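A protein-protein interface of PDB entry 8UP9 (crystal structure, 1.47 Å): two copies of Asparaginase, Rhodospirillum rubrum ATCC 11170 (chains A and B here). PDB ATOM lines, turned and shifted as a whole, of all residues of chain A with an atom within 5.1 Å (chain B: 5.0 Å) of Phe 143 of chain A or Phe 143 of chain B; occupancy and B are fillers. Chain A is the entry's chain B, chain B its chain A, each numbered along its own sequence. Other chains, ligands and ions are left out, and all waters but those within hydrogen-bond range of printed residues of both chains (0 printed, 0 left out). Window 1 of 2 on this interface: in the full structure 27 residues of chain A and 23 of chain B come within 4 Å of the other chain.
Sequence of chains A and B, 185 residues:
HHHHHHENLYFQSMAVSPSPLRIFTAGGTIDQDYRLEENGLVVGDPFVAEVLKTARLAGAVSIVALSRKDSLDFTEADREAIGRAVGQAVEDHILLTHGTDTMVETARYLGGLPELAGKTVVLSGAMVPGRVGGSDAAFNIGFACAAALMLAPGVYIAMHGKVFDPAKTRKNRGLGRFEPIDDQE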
ATOM      1  N   ALA A 138     -20.763   5.300 -16.826  1.00  0.00           N
ATOM      2  CA  ALA A 138     -19.617   5.487 -17.723  1.00  0.00           C
ATOM      3  C   ALA A 138     -19.890   4.966 -19.142  1.00  0.00           C
ATOM      4  O   ALA A 138     -19.631   5.606 -20.151  1.00  0.00           O
ATOM      5  CB  ALA A 138     -18.384   4.820 -17.168  1.00  0.00           C
ATOM      6  N   PHE A 139     -20.481   3.757 -19.214  1.00  0.00           N
ATOM      7  CA  PHE A 139     -20.920   3.236 -20.499  1.00  0.00           C
ATOM      8  C   PHE A 139     -21.881   4.225 -21.180  1.00  0.00           C
ATOM      9  O   PHE A 139     -21.760   4.517 -22.353  1.00  0.00           O
ATOM     10  CB  PHE A 139     -21.637   1.876 -20.314  1.00  0.00           C
ATOM     11  CG  PHE A 139     -22.221   1.331 -21.583  1.00  0.00           C
ATOM     12  CD1 PHE A 139     -21.498   0.507 -22.432  1.00  0.00           C
ATOM     13  CD2 PHE A 139     -23.529   1.622 -21.951  1.00  0.00           C
ATOM     14  CE1 PHE A 139     -22.041   0.084 -23.614  1.00  0.00           C
ATOM     15  CE2 PHE A 139     -24.089   1.170 -23.102  1.00  0.00           C
ATOM     16  CZ  PHE A 139     -23.345   0.358 -23.945  1.00  0.00           C
ATOM     17  N   ASN A 140     -22.905   4.702 -20.407  1.00  0.00           N
ATOM     18  CA  ASN A 140     -23.873   5.619 -21.016  1.00  0.00           C
ATOM     19  C   ASN A 140     -23.219   6.905 -21.553  1.00  0.00           C
ATOM     20  O   ASN A 140     -23.628   7.379 -22.604  1.00  0.00           O
ATOM     21  CB  ASN A 140     -24.928   5.993 -20.002  1.00  0.00           C
ATOM     22  CG  ASN A 140     -25.876   4.875 -19.637  1.00  0.00           C
ATOM     23  OD1 ASN A 140     -25.872   3.797 -20.247  1.00  0.00           O
ATOM     24  ND2 ASN A 140     -26.599   5.095 -18.540  1.00  0.00           N
ATOM     25  N   ILE A 141     -22.205   7.382 -20.851  1.00  0.00           N
ATOM     26  CA  ILE A 141     -21.508   8.598 -21.318  1.00  0.00           C
ATOM     27  C   ILE A 141     -20.727   8.350 -22.622  1.00  0.00           C
ATOM     28  O   ILE A 141     -20.859   9.098 -23.583  1.00  0.00           O
ATOM     29  CB  ILE A 141     -20.616   9.142 -20.195  1.00  0.00           C
ATOM     30  CG1 ILE A 141     -21.462   9.741 -19.066  1.00  0.00           C
ATOM     31  CG2 ILE A 141     -19.700  10.187 -20.758  1.00  0.00           C
ATOM     32  CD1 ILE A 141     -20.804   9.804 -17.724  1.00  0.00           C
ATOM     33  N   GLY A 142     -20.014   7.225 -22.678  1.00  0.00           N
ATOM     34  CA  GLY A 142     -19.339   6.908 -23.946  1.00  0.00           C
ATOM     35  C   GLY A 142     -20.325   6.783 -25.093  1.00  0.00           C
ATOM     36  O   GLY A 142     -20.102   7.287 -26.209  1.00  0.00           O
ATOM     37  N   PHE A 143     -21.416   6.004 -24.858  1.00  0.00           N
ATOM     38  CA  PHE A 143     -22.398   5.768 -25.904  1.00  0.00           C
ATOM     39  C   PHE A 143     -23.007   7.096 -26.379  1.00  0.00           C
ATOM     40  O   PHE A 143     -23.212   7.275 -27.573  1.00  0.00           O
ATOM     41  CB  PHE A 143     -23.410   4.755 -25.357  1.00  0.00           C
ATOM     42  CG  PHE A 143     -24.376   4.230 -26.393  1.00  0.00           C
ATOM     43  CD1 PHE A 143     -25.476   4.966 -26.809  1.00  0.00           C
ATOM     44  CD2 PHE A 143     -24.180   2.982 -26.990  1.00  0.00           C
ATOM     45  CE1 PHE A 143     -26.360   4.482 -27.764  1.00  0.00           C
ATOM     46  CE2 PHE A 143     -25.034   2.527 -27.972  1.00  0.00           C
ATOM     47  CZ  PHE A 143     -26.115   3.264 -28.367  1.00  0.00           C
ATOM     48  N   ALA A 144     -23.363   7.954 -25.415  1.00  0.00           N
ATOM     49  CA  ALA A 144     -24.061   9.219 -25.706  1.00  0.00           C
ATOM     50  C   ALA A 144     -23.125  10.230 -26.375  1.00  0.00           C
ATOM     51  O   ALA A 144     -23.612  10.949 -27.232  1.00  0.00           O
ATOM     52  CB  ALA A 144     -24.603   9.751 -24.430  1.00  0.00           C
ATOM     53  N   CYS A 145     -21.837  10.195 -26.064  1.00  0.00           N
ATOM     54  CA  CYS A 145     -20.853  11.058 -26.761  1.00  0.00           C
ATOM     55  C   CYS A 145     -20.811  10.647 -28.230  1.00  0.00           C
ATOM     56  O   CYS A 145     -20.860  11.512 -29.117  1.00  0.00           O
ATOM     57  CB  CYS A 145     -19.467  10.987 -26.137  1.00  0.00           C
ATOM     58  SG  CYS A 145     -19.341  11.931 -24.605  1.00  0.00           S
ATOM     59  N   ALA A 146     -20.685   9.331 -28.505  1.00  0.00           N
ATOM     60  CA  ALA A 146     -20.697   8.862 -29.897  1.00  0.00           C
ATOM     61  C   ALA A 146     -21.979   9.281 -30.597  1.00  0.00           C
ATOM     62  O   ALA A 146     -21.954   9.746 -31.734  1.00  0.00           O
ATOM     63  CB  ALA A 146     -20.489   7.364 -29.904  1.00  0.00           C
ATOM     64  N   ALA A 147     -23.131   9.072 -29.920  1.00  0.00           N
ATOM     65  CA  ALA A 147     -24.425   9.417 -30.527  1.00  0.00           C
ATOM     66  C   ALA A 147     -24.459  10.917 -30.876  1.00  0.00           C
ATOM     67  O   ALA A 147     -24.954  11.283 -31.958  1.00  0.00           O
ATOM     68  CB  ALA A 147     -25.513   8.999 -29.592  1.00  0.00           C
ATOM     69  N   LEU A 149     -22.105  12.851 -31.623  1.00  0.00           N
ATOM     70  CA  LEU A 149     -21.220  13.108 -32.786  1.00  0.00           C
ATOM     71  C   LEU A 149     -21.795  12.568 -34.084  1.00  0.00           C
ATOM     72  O   LEU A 149     -21.539  13.176 -35.121  1.00  0.00           O
ATOM     73  CB  LEU A 149     -19.836  12.528 -32.545  1.00  0.00           C
ATOM     74  CG  LEU A 149     -19.011  13.228 -31.464  1.00  0.00           C
ATOM     75  CD1 LEU A 149     -17.743  12.436 -31.212  1.00  0.00           C
ATOM     76  CD2 LEU A 149     -18.782  14.733 -31.746  1.00  0.00           C
ATOM     77  N   MET A 150     -22.435  11.395 -34.023  1.00  0.00           N
ATOM     78  CA  MET A 150     -22.752  10.599 -35.225  1.00  0.00           C
ATOM     79  C   MET A 150     -24.193  10.719 -35.698  1.00  0.00           C
ATOM     80  O   MET A 150     -24.419  10.523 -36.926  1.00  0.00           O
ATOM     81  CB  MET A 150     -22.445   9.116 -34.998  1.00  0.00           C
ATOM     82  CG  MET A 150     -21.013   8.923 -34.660  1.00  0.00           C
ATOM     83  SD  MET A 150     -20.673   7.223 -34.128  1.00  0.00           S
ATOM     84  CE  MET A 150     -18.950   7.434 -33.682  1.00  0.00           C
ATOM     85  N   ALA A 158     -30.308   8.706 -25.291  1.00  0.00           N
ATOM     86  CA  ALA A 158     -29.390   7.539 -25.489  1.00  0.00           C
ATOM     87  C   ALA A 158     -29.273   6.910 -24.110  1.00  0.00           C
ATOM     88  O   ALA A 158     -28.643   7.454 -23.206  1.00  0.00           O
ATOM     89  CB  ALA A 158     -28.093   7.986 -26.071  1.00  0.00           C
ATOM     90  N   GLY A 161     -28.000   1.387 -24.147  1.00  0.00           N
ATOM     91  CA  GLY A 161     -27.251   1.002 -25.350  1.00  0.00           C
ATOM     92  C   GLY A 161     -28.062   1.138 -26.617  1.00  0.00           C
ATOM     93  O   GLY A 161     -27.785   0.452 -27.575  1.00  0.00           O
ATOM     94  N   LYS A 162     -29.040   2.029 -26.626  1.00  0.00           N
ATOM     95  CA  LYS A 162     -29.805   2.339 -27.842  1.00  0.00           C
ATOM     96  C   LYS A 162     -30.233   3.800 -27.841  1.00  0.00           C
ATOM     97  O   LYS A 162     -30.163   4.484 -26.795  1.00  0.00           O
ATOM     98  CB  LYS A 162     -30.971   1.382 -27.946  1.00  0.00           C
ATOM     99  CG  LYS A 162     -31.983   1.520 -26.861  1.00  0.00           C
ATOM    100  CD  LYS A 162     -33.274   0.751 -27.225  1.00  0.00           C
ATOM    101  CE  LYS A 162     -34.172   1.652 -28.021  1.00  0.00           C
ATOM    102  NZ  LYS A 162     -35.360   0.922 -28.477  1.00  0.00           N
ATOM    103  N   VAL A 163     -30.758   4.165 -28.997  1.00  0.00           N
ATOM    104  CA  VAL A 163     -31.229   5.532 -29.287  1.00  0.00           C
ATOM    105  C   VAL A 163     -32.763   5.496 -29.315  1.00  0.00           C
ATOM    106  O   VAL A 163     -33.356   4.741 -30.067  1.00  0.00           O
ATOM    107  CB  VAL A 163     -30.648   6.066 -30.603  1.00  0.00           C
ATOM    108  CG1 VAL A 163     -31.191   7.433 -30.961  1.00  0.00           C
ATOM    109  CG2 VAL A 163     -29.116   6.064 -30.530  1.00  0.00           C
ATOM    110  N   PHE B 139     -15.697   3.930 -20.834  1.00  0.00           N
ATOM    111  CA  PHE B 139     -16.035   4.958 -21.819  1.00  0.00           C
ATOM    112  C   PHE B 139     -15.824   4.400 -23.221  1.00  0.00           C
ATOM    113  O   PHE B 139     -16.669   4.570 -24.112  1.00  0.00           O
ATOM    114  CB  PHE B 139     -15.169   6.203 -21.588  1.00  0.00           C
ATOM    115  CG  PHE B 139     -15.436   7.215 -22.674  1.00  0.00           C
ATOM    116  CD1 PHE B 139     -16.378   8.216 -22.510  1.00  0.00           C
ATOM    117  CD2 PHE B 139     -14.656   7.250 -23.809  1.00  0.00           C
ATOM    118  CE1 PHE B 139     -16.616   9.106 -23.544  1.00  0.00           C
ATOM    119  CE2 PHE B 139     -14.936   8.147 -24.849  1.00  0.00           C
ATOM    120  CZ  PHE B 139     -15.891   9.119 -24.703  1.00  0.00           C
ATOM    121  N   ASN B 140     -14.636   3.770 -23.436  1.00  0.00           N
ATOM    122  CA  ASN B 140     -14.324   3.326 -24.795  1.00  0.00           C
ATOM    123  C   ASN B 140     -15.324   2.266 -25.291  1.00  0.00           C
ATOM    124  O   ASN B 140     -15.692   2.279 -26.464  1.00  0.00           O
ATOM    125  CB  ASN B 140     -12.942   2.728 -24.855  1.00  0.00           C
ATOM    126  CG  ASN B 140     -11.813   3.708 -24.694  1.00  0.00           C
ATOM    127  OD1 ASN B 140     -12.017   4.939 -24.731  1.00  0.00           O
ATOM    128  ND2 ASN B 140     -10.631   3.163 -24.416  1.00  0.00           N
ATOM    129  N   ILE B 141     -15.786   1.417 -24.372  1.00  0.00           N
ATOM    130  CA  ILE B 141     -16.768   0.385 -24.758  1.00  0.00           C
ATOM    131  C   ILE B 141     -18.108   1.018 -25.139  1.00  0.00           C
ATOM    132  O   ILE B 141     -18.677   0.692 -26.142  1.00  0.00           O
ATOM    133  CB  ILE B 141     -16.865  -0.659 -23.635  1.00  0.00           C
ATOM    134  CG1 ILE B 141     -15.579  -1.514 -23.510  1.00  0.00           C
ATOM    135  CG2 ILE B 141     -18.129  -1.491 -23.877  1.00  0.00           C
ATOM    136  CD1 ILE B 141     -15.090  -2.109 -24.811  1.00  0.00           C
ATOM    137  N   GLY B 142     -18.550   1.980 -24.333  1.00  0.00           N
ATOM    138  CA  GLY B 142     -19.805   2.654 -24.685  1.00  0.00           C
ATOM    139  C   GLY B 142     -19.737   3.361 -26.017  1.00  0.00           C
ATOM    140  O   GLY B 142     -20.586   3.208 -26.894  1.00  0.00           O
ATOM    141  N   PHE B 143     -18.623   4.129 -26.206  1.00  0.00           N
ATOM    142  CA  PHE B 143     -18.434   4.865 -27.454  1.00  0.00           C
ATOM    143  C   PHE B 143     -18.350   3.900 -28.660  1.00  0.00           C
ATOM    144  O   PHE B 143     -18.931   4.156 -29.703  1.00  0.00           O
ATOM    145  CB  PHE B 143     -17.145   5.686 -27.297  1.00  0.00           C
ATOM    146  CG  PHE B 143     -16.935   6.631 -28.442  1.00  0.00           C
ATOM    147  CD1 PHE B 143     -16.326   6.237 -29.632  1.00  0.00           C
ATOM    148  CD2 PHE B 143     -17.335   7.980 -28.336  1.00  0.00           C
ATOM    149  CE1 PHE B 143     -16.155   7.121 -30.671  1.00  0.00           C
ATOM    150  CE2 PHE B 143     -17.205   8.845 -29.413  1.00  0.00           C
ATOM    151  CZ  PHE B 143     -16.608   8.413 -30.569  1.00  0.00           C
ATOM    152  N   ALA B 144     -17.597   2.763 -28.513  1.00  0.00           N
ATOM    153  CA  ALA B 144     -17.390   1.845 -29.621  1.00  0.00           C
ATOM    154  C   ALA B 144     -18.636   1.023 -29.951  1.00  0.00           C
ATOM    155  O   ALA B 144     -18.879   0.767 -31.097  1.00  0.00           O
ATOM    156  CB  ALA B 144     -16.227   0.924 -29.247  1.00  0.00           C
ATOM    157  N   CYS B 145     -19.453   0.714 -28.946  1.00  0.00           N
ATOM    158  CA  CYS B 145     -20.768   0.083 -29.213  1.00  0.00           C
ATOM    159  C   CYS B 145     -21.638   1.009 -30.081  1.00  0.00           C
ATOM    160  O   CYS B 145     -22.175   0.597 -31.080  1.00  0.00           O
ATOM    161  CB  CYS B 145     -21.533  -0.281 -27.926  1.00  0.00           C
ATOM    162  SG  CYS B 145     -20.806  -1.696 -27.048  1.00  0.00           S
ATOM    163  N   ALA B 146     -21.729   2.289 -29.654  1.00  0.00           N
ATOM    164  CA  ALA B 146     -22.486   3.248 -30.479  1.00  0.00           C
ATOM    165  C   ALA B 146     -21.918   3.344 -31.885  1.00  0.00           C
ATOM    166  O   ALA B 146     -22.669   3.350 -32.880  1.00  0.00           O
ATOM    167  CB  ALA B 146     -22.510   4.564 -29.805  1.00  0.00           C
ATOM    168  N   ALA B 147     -20.601   3.473 -31.954  1.00  0.00           N
ATOM    169  CA  ALA B 147     -19.958   3.592 -33.277  1.00  0.00           C
ATOM    170  C   ALA B 147     -20.294   2.380 -34.175  1.00  0.00           C
ATOM    171  O   ALA B 147     -20.592   2.553 -35.377  1.00  0.00           O
ATOM    172  CB  ALA B 147     -18.434   3.758 -33.136  1.00  0.00           C
ATOM    173  N   LEU B 149     -22.848   0.573 -34.152  1.00  0.00           N
ATOM    174  CA  LEU B 149     -24.290   0.666 -34.540  1.00  0.00           C
ATOM    175  C   LEU B 149     -24.577   1.763 -35.557  1.00  0.00           C
ATOM    176  O   LEU B 149     -25.495   1.587 -36.358  1.00  0.00           O
ATOM    177  CB  LEU B 149     -25.189   0.870 -33.317  1.00  0.00           C
ATOM    178  CG  LEU B 149     -25.167  -0.283 -32.331  1.00  0.00           C
ATOM    179  CD1 LEU B 149     -25.817   0.127 -31.035  1.00  0.00           C
ATOM    180  CD2 LEU B 149     -25.874  -1.515 -32.910  1.00  0.00           C
ATOM    181  N   MET B 150     -23.835   2.881 -35.479  1.00  0.00           N
ATOM    182  CA  MET B 150     -24.202   4.139 -36.184  1.00  0.00           C
ATOM    183  C   MET B 150     -23.346   4.383 -37.445  1.00  0.00           C
ATOM    184  O   MET B 150     -23.806   5.057 -38.353  1.00  0.00           O
ATOM    185  CB  MET B 150     -24.045   5.301 -35.200  1.00  0.00           C
ATOM    186  CG  MET B 150     -25.038   5.202 -34.067  1.00  0.00           C
ATOM    187  SD  MET B 150     -24.704   6.466 -32.833  1.00  0.00           S
ATOM    188  CE  MET B 150     -25.590   5.706 -31.474  1.00  0.00           C
ATOM    189  N   ALA B 158     -12.045   2.971 -32.911  1.00  0.00           N
ATOM    190  CA  ALA B 158     -12.709   3.946 -32.024  1.00  0.00           C
ATOM    191  C   ALA B 158     -11.958   4.026 -30.709  1.00  0.00           C
ATOM    192  O   ALA B 158     -11.892   3.074 -29.945  1.00  0.00           O
ATOM    193  CB  ALA B 158     -14.124   3.582 -31.807  1.00  0.00           C
ATOM    194  N   GLY B 161     -12.451   8.903 -27.916  1.00  0.00           N
ATOM    195  CA  GLY B 161     -13.743   9.518 -28.245  1.00  0.00           C
ATOM    196  C   GLY B 161     -13.844  10.001 -29.671  1.00  0.00           C
ATOM    197  O   GLY B 161     -14.604  10.987 -29.954  1.00  0.00           O
ATOM    198  N   LYS B 162     -13.158   9.329 -30.584  1.00  0.00           N
ATOM    199  CA  LYS B 162     -13.274   9.650 -32.017  1.00  0.00           C
ATOM    200  C   LYS B 162     -13.061   8.400 -32.851  1.00  0.00           C
ATOM    201  O   LYS B 162     -12.676   7.296 -32.307  1.00  0.00           O
ATOM    202  CB  LYS B 162     -12.323  10.765 -32.379  1.00  0.00           C
ATOM    203  CG  LYS B 162     -10.903  10.350 -32.247  1.00  0.00           C
ATOM    204  CD  LYS B 162      -9.991  11.259 -33.059  1.00  0.00           C
ATOM    205  CE  LYS B 162      -9.898  10.989 -34.534  1.00  0.00           C
ATOM    206  NZ  LYS B 162      -8.944  11.954 -35.100  1.00  0.00           N
ATOM    207  N   VAL B 163     -13.340   8.582 -34.098  1.00  0.00           N
ATOM    208  CA  VAL B 163     -13.234   7.509 -35.114  1.00  0.00           C
ATOM    209  C   VAL B 163     -12.008   7.736 -36.011  1.00  0.00           C
ATOM    210  O   VAL B 163     -11.892   8.799 -36.615  1.00  0.00           O
ATOM    211  CB  VAL B 163     -14.541   7.374 -35.905  1.00  0.00           C
ATOM    212  CG1 VAL B 163     -14.462   6.279 -36.929  1.00  0.00           C
ATOM    213  CG2 VAL B 163     -15.727   7.157 -34.975  1.00  0.00           C
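The backbone NH (N) of Phe 143 of chain B lies close to the backbone carbonyl oxygen (O) of Gly 142 of chain A, at 3.5 Å.
Printed residues of chain B that touch a printed residue of chain A: Phe 139, Gly 142, Phe 143, Ala 146, Ala 147, Leu 149, Met 150, Gly 161 and Val 163.
Hydrophobic or aromatic side chains of chain B within 4 Å of the printed part of chain A: Phe 139, Phe 143, Ala 146, Ala 147, Leu 149, Met 150 and Val 163.
Phe 139 of chain A touches Gly 142 of chain B, and with the chains exchanged Gly 142 of chain A touches Phe 139 of chain B.
Gly 142 of chain B touches its own counterpart, Gly 142 of chain A.
Phe 143 of chain A touches its own counterpart, Phe 143 of chain B.
Met 150 of chain A touches Val 163 of chain B, and with the chains exchanged Val 163 of chain A touches Met 150 of chain B.
Of the 17 pairs that touch across the chains among the printed residues, 15 have their exchanged pair printed and touching as well.
Of the printed residues of chain B, Phe 143 of chain A touches Gly 142 (3.3 Å), Phe 143 (3.6 Å), Ala 146 (3.6 Å), Leu 149 (3.97 Å) and Met 150 (3.98 Å).
Printed residues of chain A within 4 Å of Phe 143 of chain B: Gly 142, Phe 143 and Ala 146.
Of the printed residues of chain A, Ala 147 of chain B touches Met 150.
Printed residues of chain A within 4 Å of Val 163 of chain B: Met 150.
Printed residues of chain B within 4 Å of Leu 149 of chain A: Gly 161.
Printed residues of chain A within 4 Å of Gly 142 of chain B: Phe 139 (3.5 Å), Gly 142 (3.6 Å) and Phe 143 (3.3 Å).
Printed residues of chain B within 4 Å of Ala 147 of chain A: Met 150 (3.8 Å).
Asn 140 of chain B touches none of the printed residues of chain A.
The nearest printed residue of chain B that does not touch Phe 143 of chain A is Cys 145 of chain B (4.3 Å).
Among the printed residues, pairs that only touch across the chains: Phe 139 of chain A with Gly 142 of chain B (3.5 Å), Gly 142 of chain A with Phe 139 of chain B (3.5 Å), Gly 142 of chain A with Gly 142 of chain B (3.6 Å), Phe 143 of chain A with Gly 142 of chain B (3.3 Å), Phe 143 of chain A with Phe 143 of chain B (3.6 Å), Phe 143 of chain A with Ala 146 of chain B (3.6 Å), Phe 143 of chain A with Leu 149 of chain B (3.97 Å), Phe 143 of chain A with Met 150 of chain B (3.98 Å), Ala 146 of chain A with Phe 143 of chain B (3.5 Å), Ala 146 of chain A with Ala 146 of chain B (3.5 Å), Ala 147 of chain A with Met 150 of chain B (3.8 Å), Leu 149 of chain A with Gly 161 of chain B (3.7 Å), Met 150 of chain A with Ala 147 of chain B (3.8 Å), Met 150 of chain A with Val 163 of chain B (3.5 Å), Gly 161 of chain A with Leu 149 of chain B (3.99 Å) and Val 163 of chain A with Met 150 of chain B (3.7 Å).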
